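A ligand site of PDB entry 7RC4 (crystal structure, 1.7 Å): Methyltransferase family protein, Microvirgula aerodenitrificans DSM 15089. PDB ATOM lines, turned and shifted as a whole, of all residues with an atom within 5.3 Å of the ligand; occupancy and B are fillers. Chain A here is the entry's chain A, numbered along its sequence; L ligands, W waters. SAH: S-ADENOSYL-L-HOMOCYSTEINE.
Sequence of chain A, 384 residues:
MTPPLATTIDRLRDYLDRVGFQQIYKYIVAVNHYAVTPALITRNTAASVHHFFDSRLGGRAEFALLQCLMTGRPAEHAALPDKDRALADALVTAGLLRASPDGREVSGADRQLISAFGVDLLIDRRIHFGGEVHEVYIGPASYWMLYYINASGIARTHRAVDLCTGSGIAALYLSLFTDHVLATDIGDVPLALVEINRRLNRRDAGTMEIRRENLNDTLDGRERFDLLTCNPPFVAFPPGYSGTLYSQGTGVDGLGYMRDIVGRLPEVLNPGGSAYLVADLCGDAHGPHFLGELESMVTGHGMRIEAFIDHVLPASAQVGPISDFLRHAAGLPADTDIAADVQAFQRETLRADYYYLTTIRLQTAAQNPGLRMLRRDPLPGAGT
The side-chain hydroxyl of Ser 142 sits at hydrogen-bond distance from an oxygen (O) of the ligand, 2.6 Å away. An oxygen (OXT) of the ligand lies within hydrogen-bond range of the side-chain amide nitrogen (ND2) of Asn 231 (3.1 Å). O of Cys 164 is in hydrogen-bond range of N of the ligand, 2.8 Å away. N of the ligand sits close to O of Thr 165, 3.4 Å away. The backbone NH (N) of Leu 215 lies within hydrogen-bond range of a nitrogen (N1) of the ligand, 2.9 Å away. The side-chain sulfur (SG) of Cys 164 lies within hydrogen-bond range of a nitrogen (N3) of the ligand (3.5 Å). The side-chain carboxylate (OD1) of Asp 185 sits at hydrogen-bond distance from an oxygen (O2') of the ligand, at 2.6 Å. OH of Tyr 257 lies within hydrogen-bond range of N6 of the ligand (3.2 Å).
OD2 of Asp 185 lies within hydrogen-bond range of N of Thr 165 (3.5 Å). The side-chain hydroxyl (OG) of Ser 142 sits at hydrogen-bond distance from the backbone NH (N) of Gly 139, at 3.0 Å. The side-chain carboxylate (OD2) of Asp 185 sits at hydrogen-bond distance from the backbone NH (N) of Gly 166. OG of Ser 167 lies within hydrogen-bond range of N of Ile 169 (3.4 Å). The backbone NH of Glu 213 sits at hydrogen-bond distance from the backbone carbonyl oxygen of Asp 185, 3.1 Å away. The side-chain hydroxyl (OH) of Tyr 137 sits close to the backbone NH (N) of Gly 139. The side-chain carboxylate (OD1) of Asp 185 lies within hydrogen-bond range of the backbone NH (N) of Gly 187 (3.0 Å). The backbone NH (N) of Thr 165 lies within hydrogen-bond range of the backbone carbonyl oxygen (O) of Thr 184, at 2.7 Å.
Tyr 137 touches the ligand. CG1 of Ile 138 touches O of the ligand (3.9 Å). CA of Gly 166 touches O3' of the ligand, at 3.3 Å. Ile 169 touches the ligand (CG2 to O, 3.9 Å). Ile 186 touches the ligand. Pro 190 touches the ligand (CG to O2', 3.8 Å). O of Glu 213 touches C2 of the ligand (3.6 Å). Asn 214 touches the ligand. CG of Pro 233 touches C8 of the ligand (3.3 Å). O of Leu 245 touches C8 of the ligand (3.4 Å). Tyr 246 touches the ligand (CB to C3', 3.8 Å). Hydrophobic or aromatic side chains that line the ligand: Tyr 137, Ile 138, Ile 169, Ile 186, Pro 190, Leu 215, Pro 233, Leu 245, Tyr 246 and Tyr 257. The nearest printed residue that does not touch the ligand is Gly 187 (4.2 Å).
Water W1 lies within hydrogen-bond range of OD2 of Asp 162 (2.7 Å), O of Thr 165 (2.7 Å), N of the ligand (2.8 Å) and N of Ala 170 (3.0 Å). Water W3 lies within hydrogen-bond range of the side-chain hydroxyl (OG) of Ser 167, the backbone carbonyl oxygen (O) of Tyr 137 and an oxygen (O) of the ligand. Water W4 bridges an oxygen (O3') of the ligand and the backbone NH (N) of Tyr 137. Water W5 bridges OH of Tyr 257 (2.6 Å) and N7 of the ligand (2.8 Å). Water W6 bridges an oxygen (OXT) of the ligand (3.0 Å) and the backbone carbonyl oxygen of Ser 142 (3.0 Å). Water W8 bridges O of Tyr 246 and SD of the ligand.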
ATOM      1  N   TYR A 137      -6.529 -17.671  13.708  1.00  0.00           N
ATOM      2  CA  TYR A 137      -6.963 -17.605  12.321  1.00  0.00           C
ATOM      3  C   TYR A 137      -6.600 -18.892  11.580  1.00  0.00           C
ATOM      4  O   TYR A 137      -5.551 -19.478  11.808  1.00  0.00           O
ATOM      5  CB  TYR A 137      -6.297 -16.419  11.615  1.00  0.00           C
ATOM      6  CG  TYR A 137      -6.273 -16.556  10.112  1.00  0.00           C
ATOM      7  CD1 TYR A 137      -7.332 -16.104   9.340  1.00  0.00           C
ATOM      8  CD2 TYR A 137      -5.201 -17.174   9.462  1.00  0.00           C
ATOM      9  CE1 TYR A 137      -7.324 -16.242   7.957  1.00  0.00           C
ATOM     10  CE2 TYR A 137      -5.184 -17.321   8.105  1.00  0.00           C
ATOM     11  CZ  TYR A 137      -6.233 -16.858   7.353  1.00  0.00           C
ATOM     12  OH  TYR A 137      -6.181 -17.027   5.988  1.00  0.00           O
ATOM     13  N   ILE A 138      -7.490 -19.288  10.674  1.00  0.00           N
ATOM     14  CA  ILE A 138      -7.146 -20.129   9.522  1.00  0.00           C
ATOM     15  C   ILE A 138      -8.127 -19.760   8.412  1.00  0.00           C
ATOM     16  O   ILE A 138      -9.245 -19.327   8.688  1.00  0.00           O
ATOM     17  CB  ILE A 138      -7.168 -21.639   9.863  1.00  0.00           C
ATOM     18  CG1 ILE A 138      -6.435 -22.455   8.793  1.00  0.00           C
ATOM     19  CG2 ILE A 138      -8.605 -22.138  10.077  1.00  0.00           C
ATOM     20  CD1 ILE A 138      -6.287 -23.922   9.172  1.00  0.00           C
ATOM     21  N   GLY A 139      -7.689 -19.855   7.173  1.00  0.00           N
ATOM     22  CA  GLY A 139      -8.565 -19.469   6.081  1.00  0.00           C
ATOM     23  C   GLY A 139      -8.052 -19.985   4.758  1.00  0.00           C
ATOM     24  O   GLY A 139      -7.047 -20.698   4.685  1.00  0.00           O
ATOM     25  N   SER A 142      -4.375 -19.550   3.970  1.00  0.00           N
ATOM     26  CA  SER A 142      -3.516 -20.592   4.542  1.00  0.00           C
ATOM     27  C   SER A 142      -3.344 -21.749   3.563  1.00  0.00           C
ATOM     28  O   SER A 142      -2.220 -22.225   3.352  1.00  0.00           O
ATOM     29  CB  SER A 142      -4.125 -21.138   5.860  1.00  0.00           C
ATOM     30  OG  SER A 142      -4.701 -20.120   6.688  1.00  0.00           O
ATOM     31  N   MET A 145      -1.401 -20.770   0.021  1.00  0.00           N
ATOM     32  CA  MET A 145       0.037 -20.779   0.286  1.00  0.00           C
ATOM     33  C   MET A 145       0.648 -22.161   0.118  1.00  0.00           C
ATOM     34  O   MET A 145       1.668 -22.335  -0.548  1.00  0.00           O
ATOM     35  CB  MET A 145       0.328 -20.283   1.700  1.00  0.00           C
ATOM     36  CG  MET A 145       1.774 -19.901   1.891  1.00  0.00           C
ATOM     37  SD  MET A 145       2.085 -19.207   3.525  1.00  0.00           S
ATOM     38  CE  MET A 145       1.581 -20.549   4.599  1.00  0.00           C
ATOM     39  N   ASP A 162       8.351 -22.013   9.264  1.00  0.00           N
ATOM     40  CA  ASP A 162       7.009 -21.447   9.106  1.00  0.00           C
ATOM     41  C   ASP A 162       6.880 -20.312  10.118  1.00  0.00           C
ATOM     42  O   ASP A 162       6.679 -20.555  11.316  1.00  0.00           O
ATOM     43  CB  ASP A 162       5.933 -22.495   9.365  1.00  0.00           C
ATOM     44  CG  ASP A 162       4.528 -21.935   9.193  1.00  0.00           C
ATOM     45  OD1 ASP A 162       4.325 -21.073   8.318  1.00  0.00           O
ATOM     46  OD2 ASP A 162       3.622 -22.358   9.949  1.00  0.00           O
ATOM     47  N   LEU A 163       6.998 -19.078   9.632  1.00  0.00           N
ATOM     48  CA  LEU A 163       6.841 -17.899  10.483  1.00  0.00           C
ATOM     49  C   LEU A 163       5.368 -17.587  10.677  1.00  0.00           C
ATOM     50  O   LEU A 163       4.565 -17.699   9.743  1.00  0.00           O
ATOM     51  CB  LEU A 163       7.527 -16.692   9.853  1.00  0.00           C
ATOM     52  CG  LEU A 163       9.004 -16.839   9.520  1.00  0.00           C
ATOM     53  CD1 LEU A 163       9.429 -15.752   8.545  1.00  0.00           C
ATOM     54  CD2 LEU A 163       9.796 -16.762  10.806  1.00  0.00           C
ATOM     55  N   CYS A 164       5.000 -17.161  11.900  1.00  0.00           N
ATOM     56  CA  CYS A 164       3.620 -16.769  12.202  1.00  0.00           C
ATOM     57  C   CYS A 164       2.673 -17.952  12.022  1.00  0.00           C
ATOM     58  O   CYS A 164       1.692 -17.895  11.269  1.00  0.00           O
ATOM     59  CB  CYS A 164       3.163 -15.591  11.329  1.00  0.00           C
ATOM     60  SG  CYS A 164       4.215 -14.138  11.287  1.00  0.00           S
ATOM     61  N   THR A 165       2.969 -19.029  12.751  1.00  0.00           N
ATOM     62  CA  THR A 165       2.434 -20.353  12.429  1.00  0.00           C
ATOM     63  C   THR A 165       0.946 -20.533  12.801  1.00  0.00           C
ATOM     64  O   THR A 165       0.282 -21.375  12.190  1.00  0.00           O
ATOM     65  CB  THR A 165       3.308 -21.417  13.100  1.00  0.00           C
ATOM     66  OG1 THR A 165       3.048 -22.693  12.501  1.00  0.00           O
ATOM     67  CG2 THR A 165       3.027 -21.517  14.636  1.00  0.00           C
ATOM     68  N   GLY A 166       0.421 -19.758  13.749  1.00  0.00           N
ATOM     69  CA  GLY A 166      -1.002 -19.887  14.076  1.00  0.00           C
ATOM     70  C   GLY A 166      -1.355 -21.268  14.605  1.00  0.00           C
ATOM     71  O   GLY A 166      -0.758 -21.752  15.581  1.00  0.00           O
ATOM     72  N   SER A 167      -2.313 -21.927  13.955  1.00  0.00           N
ATOM     73  CA  SER A 167      -2.674 -23.308  14.289  1.00  0.00           C
ATOM     74  C   SER A 167      -1.538 -24.299  14.068  1.00  0.00           C
ATOM     75  O   SER A 167      -1.560 -25.408  14.626  1.00  0.00           O
ATOM     76  CB  SER A 167      -3.888 -23.754  13.454  1.00  0.00           C
ATOM     77  OG  SER A 167      -3.532 -23.893  12.074  1.00  0.00           O
ATOM     78  N   ILE A 169      -0.627 -25.208  10.802  1.00  0.00           N
ATOM     79  CA  ILE A 169      -0.920 -25.965   9.578  1.00  0.00           C
ATOM     80  C   ILE A 169       0.286 -25.999   8.627  1.00  0.00           C
ATOM     81  O   ILE A 169       0.669 -27.058   8.136  1.00  0.00           O
ATOM     82  CB  ILE A 169      -2.185 -25.428   8.893  1.00  0.00           C
ATOM     83  CG1 ILE A 169      -2.456 -26.206   7.606  1.00  0.00           C
ATOM     84  CG2 ILE A 169      -2.117 -23.903   8.665  1.00  0.00           C
ATOM     85  CD1 ILE A 169      -3.669 -25.702   6.850  1.00  0.00           C
ATOM     86  N   ALA A 170       0.900 -24.845   8.356  1.00  0.00           N
ATOM     87  CA  ALA A 170       1.992 -24.845   7.381  1.00  0.00           C
ATOM     88  C   ALA A 170       3.199 -25.615   7.899  1.00  0.00           C
ATOM     89  O   ALA A 170       3.815 -26.391   7.169  1.00  0.00           O
ATOM     90  CB  ALA A 170       2.382 -23.412   7.004  1.00  0.00           C
ATOM     91  N   THR A 184       7.078 -20.530  14.391  1.00  0.00           N
ATOM     92  CA  THR A 184       7.144 -19.401  15.327  1.00  0.00           C
ATOM     93  C   THR A 184       5.819 -18.682  15.449  1.00  0.00           C
ATOM     94  O   THR A 184       5.022 -18.637  14.506  1.00  0.00           O
ATOM     95  CB  THR A 184       8.194 -18.349  14.900  1.00  0.00           C
ATOM     96  OG1 THR A 184       7.726 -17.633  13.754  1.00  0.00           O
ATOM     97  CG2 THR A 184       9.533 -18.989  14.579  1.00  0.00           C
ATOM     98  N   ASP A 185       5.589 -18.092  16.624  1.00  0.00           N
ATOM     99  CA  ASP A 185       4.448 -17.206  16.832  1.00  0.00           C
ATOM    100  C   ASP A 185       4.727 -16.414  18.103  1.00  0.00           C
ATOM    101  O   ASP A 185       5.722 -16.660  18.787  1.00  0.00           O
ATOM    102  CB  ASP A 185       3.126 -17.998  16.931  1.00  0.00           C
ATOM    103  CG  ASP A 185       1.910 -17.191  16.452  1.00  0.00           C
ATOM    104  OD1 ASP A 185       1.561 -16.174  17.095  1.00  0.00           O
ATOM    105  OD2 ASP A 185       1.285 -17.583  15.431  1.00  0.00           O
ATOM    106  N   ILE A 186       3.861 -15.439  18.397  1.00  0.00           N
ATOM    107  CA  ILE A 186       4.021 -14.677  19.639  1.00  0.00           C
ATOM    108  C   ILE A 186       2.734 -14.677  20.464  1.00  0.00           C
ATOM    109  O   ILE A 186       2.723 -14.182  21.594  1.00  0.00           O
ATOM    110  CB  ILE A 186       4.487 -13.231  19.381  1.00  0.00           C
ATOM    111  CG1 ILE A 186       3.487 -12.468  18.523  1.00  0.00           C
ATOM    112  CG2 ILE A 186       5.877 -13.237  18.756  1.00  0.00           C
ATOM    113  CD1 ILE A 186       3.881 -11.019  18.246  1.00  0.00           C
ATOM    114  N   GLY A 187       1.645 -15.212  19.918  1.00  0.00           N
ATOM    115  CA  GLY A 187       0.380 -15.241  20.644  1.00  0.00           C
ATOM    116  C   GLY A 187       0.279 -16.435  21.563  1.00  0.00           C
ATOM    117  O   GLY A 187       0.553 -17.570  21.156  1.00  0.00           O
ATOM    118  N   PRO A 190      -2.400 -19.117  19.952  1.00  0.00           N
ATOM    119  CA  PRO A 190      -1.868 -19.975  18.872  1.00  0.00           C
ATOM    120  C   PRO A 190      -0.693 -20.841  19.303  1.00  0.00           C
ATOM    121  O   PRO A 190      -0.600 -22.001  18.867  1.00  0.00           O
ATOM    122  CB  PRO A 190      -1.457 -18.967  17.777  1.00  0.00           C
ATOM    123  CG  PRO A 190      -1.382 -17.642  18.442  1.00  0.00           C
ATOM    124  CD  PRO A 190      -2.430 -17.699  19.537  1.00  0.00           C
ATOM    125  N   GLU A 213       8.697 -16.129  19.273  1.00  0.00           N
ATOM    126  CA  GLU A 213       9.684 -15.191  18.737  1.00  0.00           C
ATOM    127  C   GLU A 213       9.043 -14.279  17.698  1.00  0.00           C
ATOM    128  O   GLU A 213       8.288 -14.746  16.833  1.00  0.00           O
ATOM    129  CB  GLU A 213      10.867 -15.947  18.134  1.00  0.00           C
ATOM    130  CG  GLU A 213      11.981 -15.070  17.612  1.00  0.00           C
ATOM    131  CD  GLU A 213      13.250 -15.869  17.380  1.00  0.00           C
ATOM    132  OE1 GLU A 213      13.343 -16.534  16.332  1.00  0.00           O
ATOM    133  OE2 GLU A 213      14.130 -15.836  18.259  1.00  0.00           O
ATOM    134  N   ASN A 214       9.359 -12.988  17.789  1.00  0.00           N
ATOM    135  CA  ASN A 214       8.893 -12.003  16.810  1.00  0.00           C
ATOM    136  C   ASN A 214       9.469 -12.312  15.429  1.00  0.00           C
ATOM    137  O   ASN A 214      10.624 -12.692  15.304  1.00  0.00           O
ATOM    138  CB  ASN A 214       9.343 -10.592  17.196  1.00  0.00           C
ATOM    139  CG  ASN A 214       8.751 -10.085  18.494  1.00  0.00           C
ATOM    140  OD1 ASN A 214       7.560 -10.219  18.744  1.00  0.00           O
ATOM    141  ND2 ASN A 214       9.594  -9.436  19.310  1.00  0.00           N
ATOM    142  N   LEU A 215       8.621 -12.130  14.403  1.00  0.00           N
ATOM    143  CA  LEU A 215       9.033 -12.337  13.017  1.00  0.00           C
ATOM    144  C   LEU A 215      10.349 -11.636  12.694  1.00  0.00           C
ATOM    145  O   LEU A 215      11.247 -12.230  12.100  1.00  0.00           O
ATOM    146  CB  LEU A 215       7.890 -11.856  12.084  1.00  0.00           C
ATOM    147  CG  LEU A 215       7.961 -11.689  10.569  1.00  0.00           C
ATOM    148  CD1 LEU A 215       6.559 -11.570  10.018  1.00  0.00           C
ATOM    149  CD2 LEU A 215       8.624 -10.387  10.300  1.00  0.00           C
ATOM    150  N   ASN A 231       2.283 -16.681   6.203  1.00  0.00           N
ATOM    151  CA  ASN A 231       1.014 -15.981   6.035  1.00  0.00           C
ATOM    152  C   ASN A 231       0.940 -14.986   7.202  1.00  0.00           C
ATOM    153  O   ASN A 231       0.429 -15.335   8.277  1.00  0.00           O
ATOM    154  CB  ASN A 231      -0.147 -16.975   6.067  1.00  0.00           C
ATOM    155  CG  ASN A 231      -1.504 -16.321   5.920  1.00  0.00           C
ATOM    156  OD1 ASN A 231      -1.625 -15.100   5.774  1.00  0.00           O
ATOM    157  ND2 ASN A 231      -2.548 -17.139   5.953  1.00  0.00           N
ATOM    158  N   PRO A 232       1.476 -13.777   7.051  1.00  0.00           N
ATOM    159  CA  PRO A 232       1.582 -12.857   8.189  1.00  0.00           C
ATOM    160  C   PRO A 232       0.317 -12.041   8.332  1.00  0.00           C
ATOM    161  O   PRO A 232      -0.532 -12.022   7.423  1.00  0.00           O
ATOM    162  CB  PRO A 232       2.764 -11.968   7.781  1.00  0.00           C
ATOM    163  CG  PRO A 232       2.572 -11.832   6.292  1.00  0.00           C
ATOM    164  CD  PRO A 232       2.087 -13.206   5.835  1.00  0.00           C
ATOM    165  N   PRO A 233       0.128 -11.344   9.461  1.00  0.00           N
ATOM    166  CA  PRO A 233      -0.896 -10.291   9.502  1.00  0.00           C
ATOM    167  C   PRO A 233      -0.652  -9.315   8.360  1.00  0.00           C
ATOM    168  O   PRO A 233       0.450  -8.784   8.204  1.00  0.00           O
ATOM    169  CB  PRO A 233      -0.696  -9.641  10.872  1.00  0.00           C
ATOM    170  CG  PRO A 233       0.059 -10.643  11.688  1.00  0.00           C
ATOM    171  CD  PRO A 233       0.938 -11.383  10.684  1.00  0.00           C
ATOM    172  N   LEU A 245      -4.364  -9.598  16.742  1.00  0.00           N
ATOM    173  CA  LEU A 245      -2.979 -10.024  16.518  1.00  0.00           C
ATOM    174  C   LEU A 245      -2.822 -10.716  15.172  1.00  0.00           C
ATOM    175  O   LEU A 245      -1.819 -10.509  14.473  1.00  0.00           O
ATOM    176  CB  LEU A 245      -2.545 -10.945  17.658  1.00  0.00           C
ATOM    177  CG  LEU A 245      -1.098 -11.434  17.681  1.00  0.00           C
ATOM    178  CD1 LEU A 245      -0.127 -10.247  17.746  1.00  0.00           C
ATOM    179  CD2 LEU A 245      -0.890 -12.376  18.861  1.00  0.00           C
ATOM    180  N   TYR A 246      -3.784 -11.548  14.778  1.00  0.00           N
ATOM    181  CA  TYR A 246      -3.604 -12.291  13.527  1.00  0.00           C
ATOM    182  C   TYR A 246      -3.953 -11.496  12.280  1.00  0.00           C
ATOM    183  O   TYR A 246      -3.517 -11.871  11.179  1.00  0.00           O
ATOM    184  CB  TYR A 246      -4.448 -13.583  13.527  1.00  0.00           C
ATOM    185  CG  TYR A 246      -5.899 -13.378  13.875  1.00  0.00           C
ATOM    186  CD1 TYR A 246      -6.820 -12.992  12.911  1.00  0.00           C
ATOM    187  CD2 TYR A 246      -6.353 -13.602  15.177  1.00  0.00           C
ATOM    188  CE1 TYR A 246      -8.159 -12.798  13.239  1.00  0.00           C
ATOM    189  CE2 TYR A 246      -7.674 -13.414  15.516  1.00  0.00           C
ATOM    190  CZ  TYR A 246      -8.575 -13.012  14.554  1.00  0.00           C
ATOM    191  OH  TYR A 246      -9.900 -12.838  14.923  1.00  0.00           O
ATOM    192  N   TYR A 257       4.916  -6.225   7.284  1.00  0.00           N
ATOM    193  CA  TYR A 257       5.525  -7.523   7.582  1.00  0.00           C
ATOM    194  C   TYR A 257       5.949  -8.209   6.288  1.00  0.00           C
ATOM    195  O   TYR A 257       6.996  -8.883   6.248  1.00  0.00           O
ATOM    196  CB  TYR A 257       4.543  -8.413   8.356  1.00  0.00           C
ATOM    197  CG  TYR A 257       4.397  -8.100   9.838  1.00  0.00           C
ATOM    198  CD1 TYR A 257       5.485  -7.748  10.639  1.00  0.00           C
ATOM    199  CD2 TYR A 257       3.148  -8.179  10.444  1.00  0.00           C
ATOM    200  CE1 TYR A 257       5.312  -7.487  12.011  1.00  0.00           C
ATOM    201  CE2 TYR A 257       2.974  -7.919  11.816  1.00  0.00           C
ATOM    202  CZ  TYR A 257       4.059  -7.576  12.588  1.00  0.00           C
ATOM    203  OH  TYR A 257       3.881  -7.325  13.932  1.00  0.00           O
HETATM  204  N   SAH L   1       0.263 -19.503   9.402  1.00  0.00           N
HETATM  205  CA  SAH L   1      -1.122 -19.621   9.872  1.00  0.00           C
HETATM  206  CB  SAH L   1      -1.557 -18.389  10.689  1.00  0.00           C
HETATM  207  CG  SAH L   1      -1.440 -17.029  10.006  1.00  0.00           C
HETATM  208  SD  SAH L   1      -2.372 -15.737  10.898  1.00  0.00           S
HETATM  209  C   SAH L   1      -2.029 -19.837   8.665  1.00  0.00           C
HETATM  210  O   SAH L   1      -3.192 -20.207   8.821  1.00  0.00           O
HETATM  211  OXT SAH L   1      -1.607 -19.672   7.509  1.00  0.00           O
HETATM  212  C5' SAH L   1      -0.917 -14.750  11.392  1.00  0.00           C
HETATM  213  C4' SAH L   1      -0.226 -15.197  12.681  1.00  0.00           C
HETATM  214  O4' SAH L   1       0.804 -14.282  13.015  1.00  0.00           O
HETATM  215  C3' SAH L   1      -1.097 -15.250  13.952  1.00  0.00           C
HETATM  216  O3' SAH L   1      -1.064 -16.569  14.461  1.00  0.00           O
HETATM  217  C2' SAH L   1      -0.437 -14.276  14.920  1.00  0.00           C
HETATM  218  O2' SAH L   1      -0.418 -14.679  16.283  1.00  0.00           O
HETATM  219  C1' SAH L   1       0.994 -14.259  14.431  1.00  0.00           C
HETATM  220  N9  SAH L   1       1.763 -13.030  14.610  1.00  0.00           N
HETATM  221  C8  SAH L   1       1.299 -11.730  14.575  1.00  0.00           C
HETATM  222  N7  SAH L   1       2.364 -10.906  14.698  1.00  0.00           N
HETATM  223  C5  SAH L   1       3.495 -11.648  14.775  1.00  0.00           C
HETATM  224  C6  SAH L   1       4.851 -11.315  14.879  1.00  0.00           C
HETATM  225  N6  SAH L   1       5.254 -10.031  14.949  1.00  0.00           N
HETATM  226  N1  SAH L   1       5.777 -12.318  14.955  1.00  0.00           N
HETATM  227  C2  SAH L   1       5.398 -13.649  14.901  1.00  0.00           C
HETATM  228  N3  SAH L   1       4.055 -13.978  14.794  1.00  0.00           N
HETATM  229  C4  SAH L   1       3.132 -12.984  14.717  1.00  0.00           C
HETATM  230  O   HOH W   1       0.975 -22.205   9.712  1.00  0.00           O
HETATM  231  O   HOH W   2       2.631 -18.904   8.222  1.00  0.00           O
HETATM  232  O   HOH W   3      -3.736 -21.360  11.329  1.00  0.00           O
HETATM  233  O   HOH W   4      -3.836 -16.886  14.886  1.00  0.00           O
HETATM  234  O   HOH W   5       1.703  -8.163  15.088  1.00  0.00           O
HETATM  235  O   HOH W   6      -0.819 -22.158   6.033  1.00  0.00           O
HETATM  236  O   HOH W   7      -3.278 -14.729  16.715  1.00  0.00           O
HETATM  237  O   HOH W   8      -4.393 -13.592   9.318  1.00  0.00           O
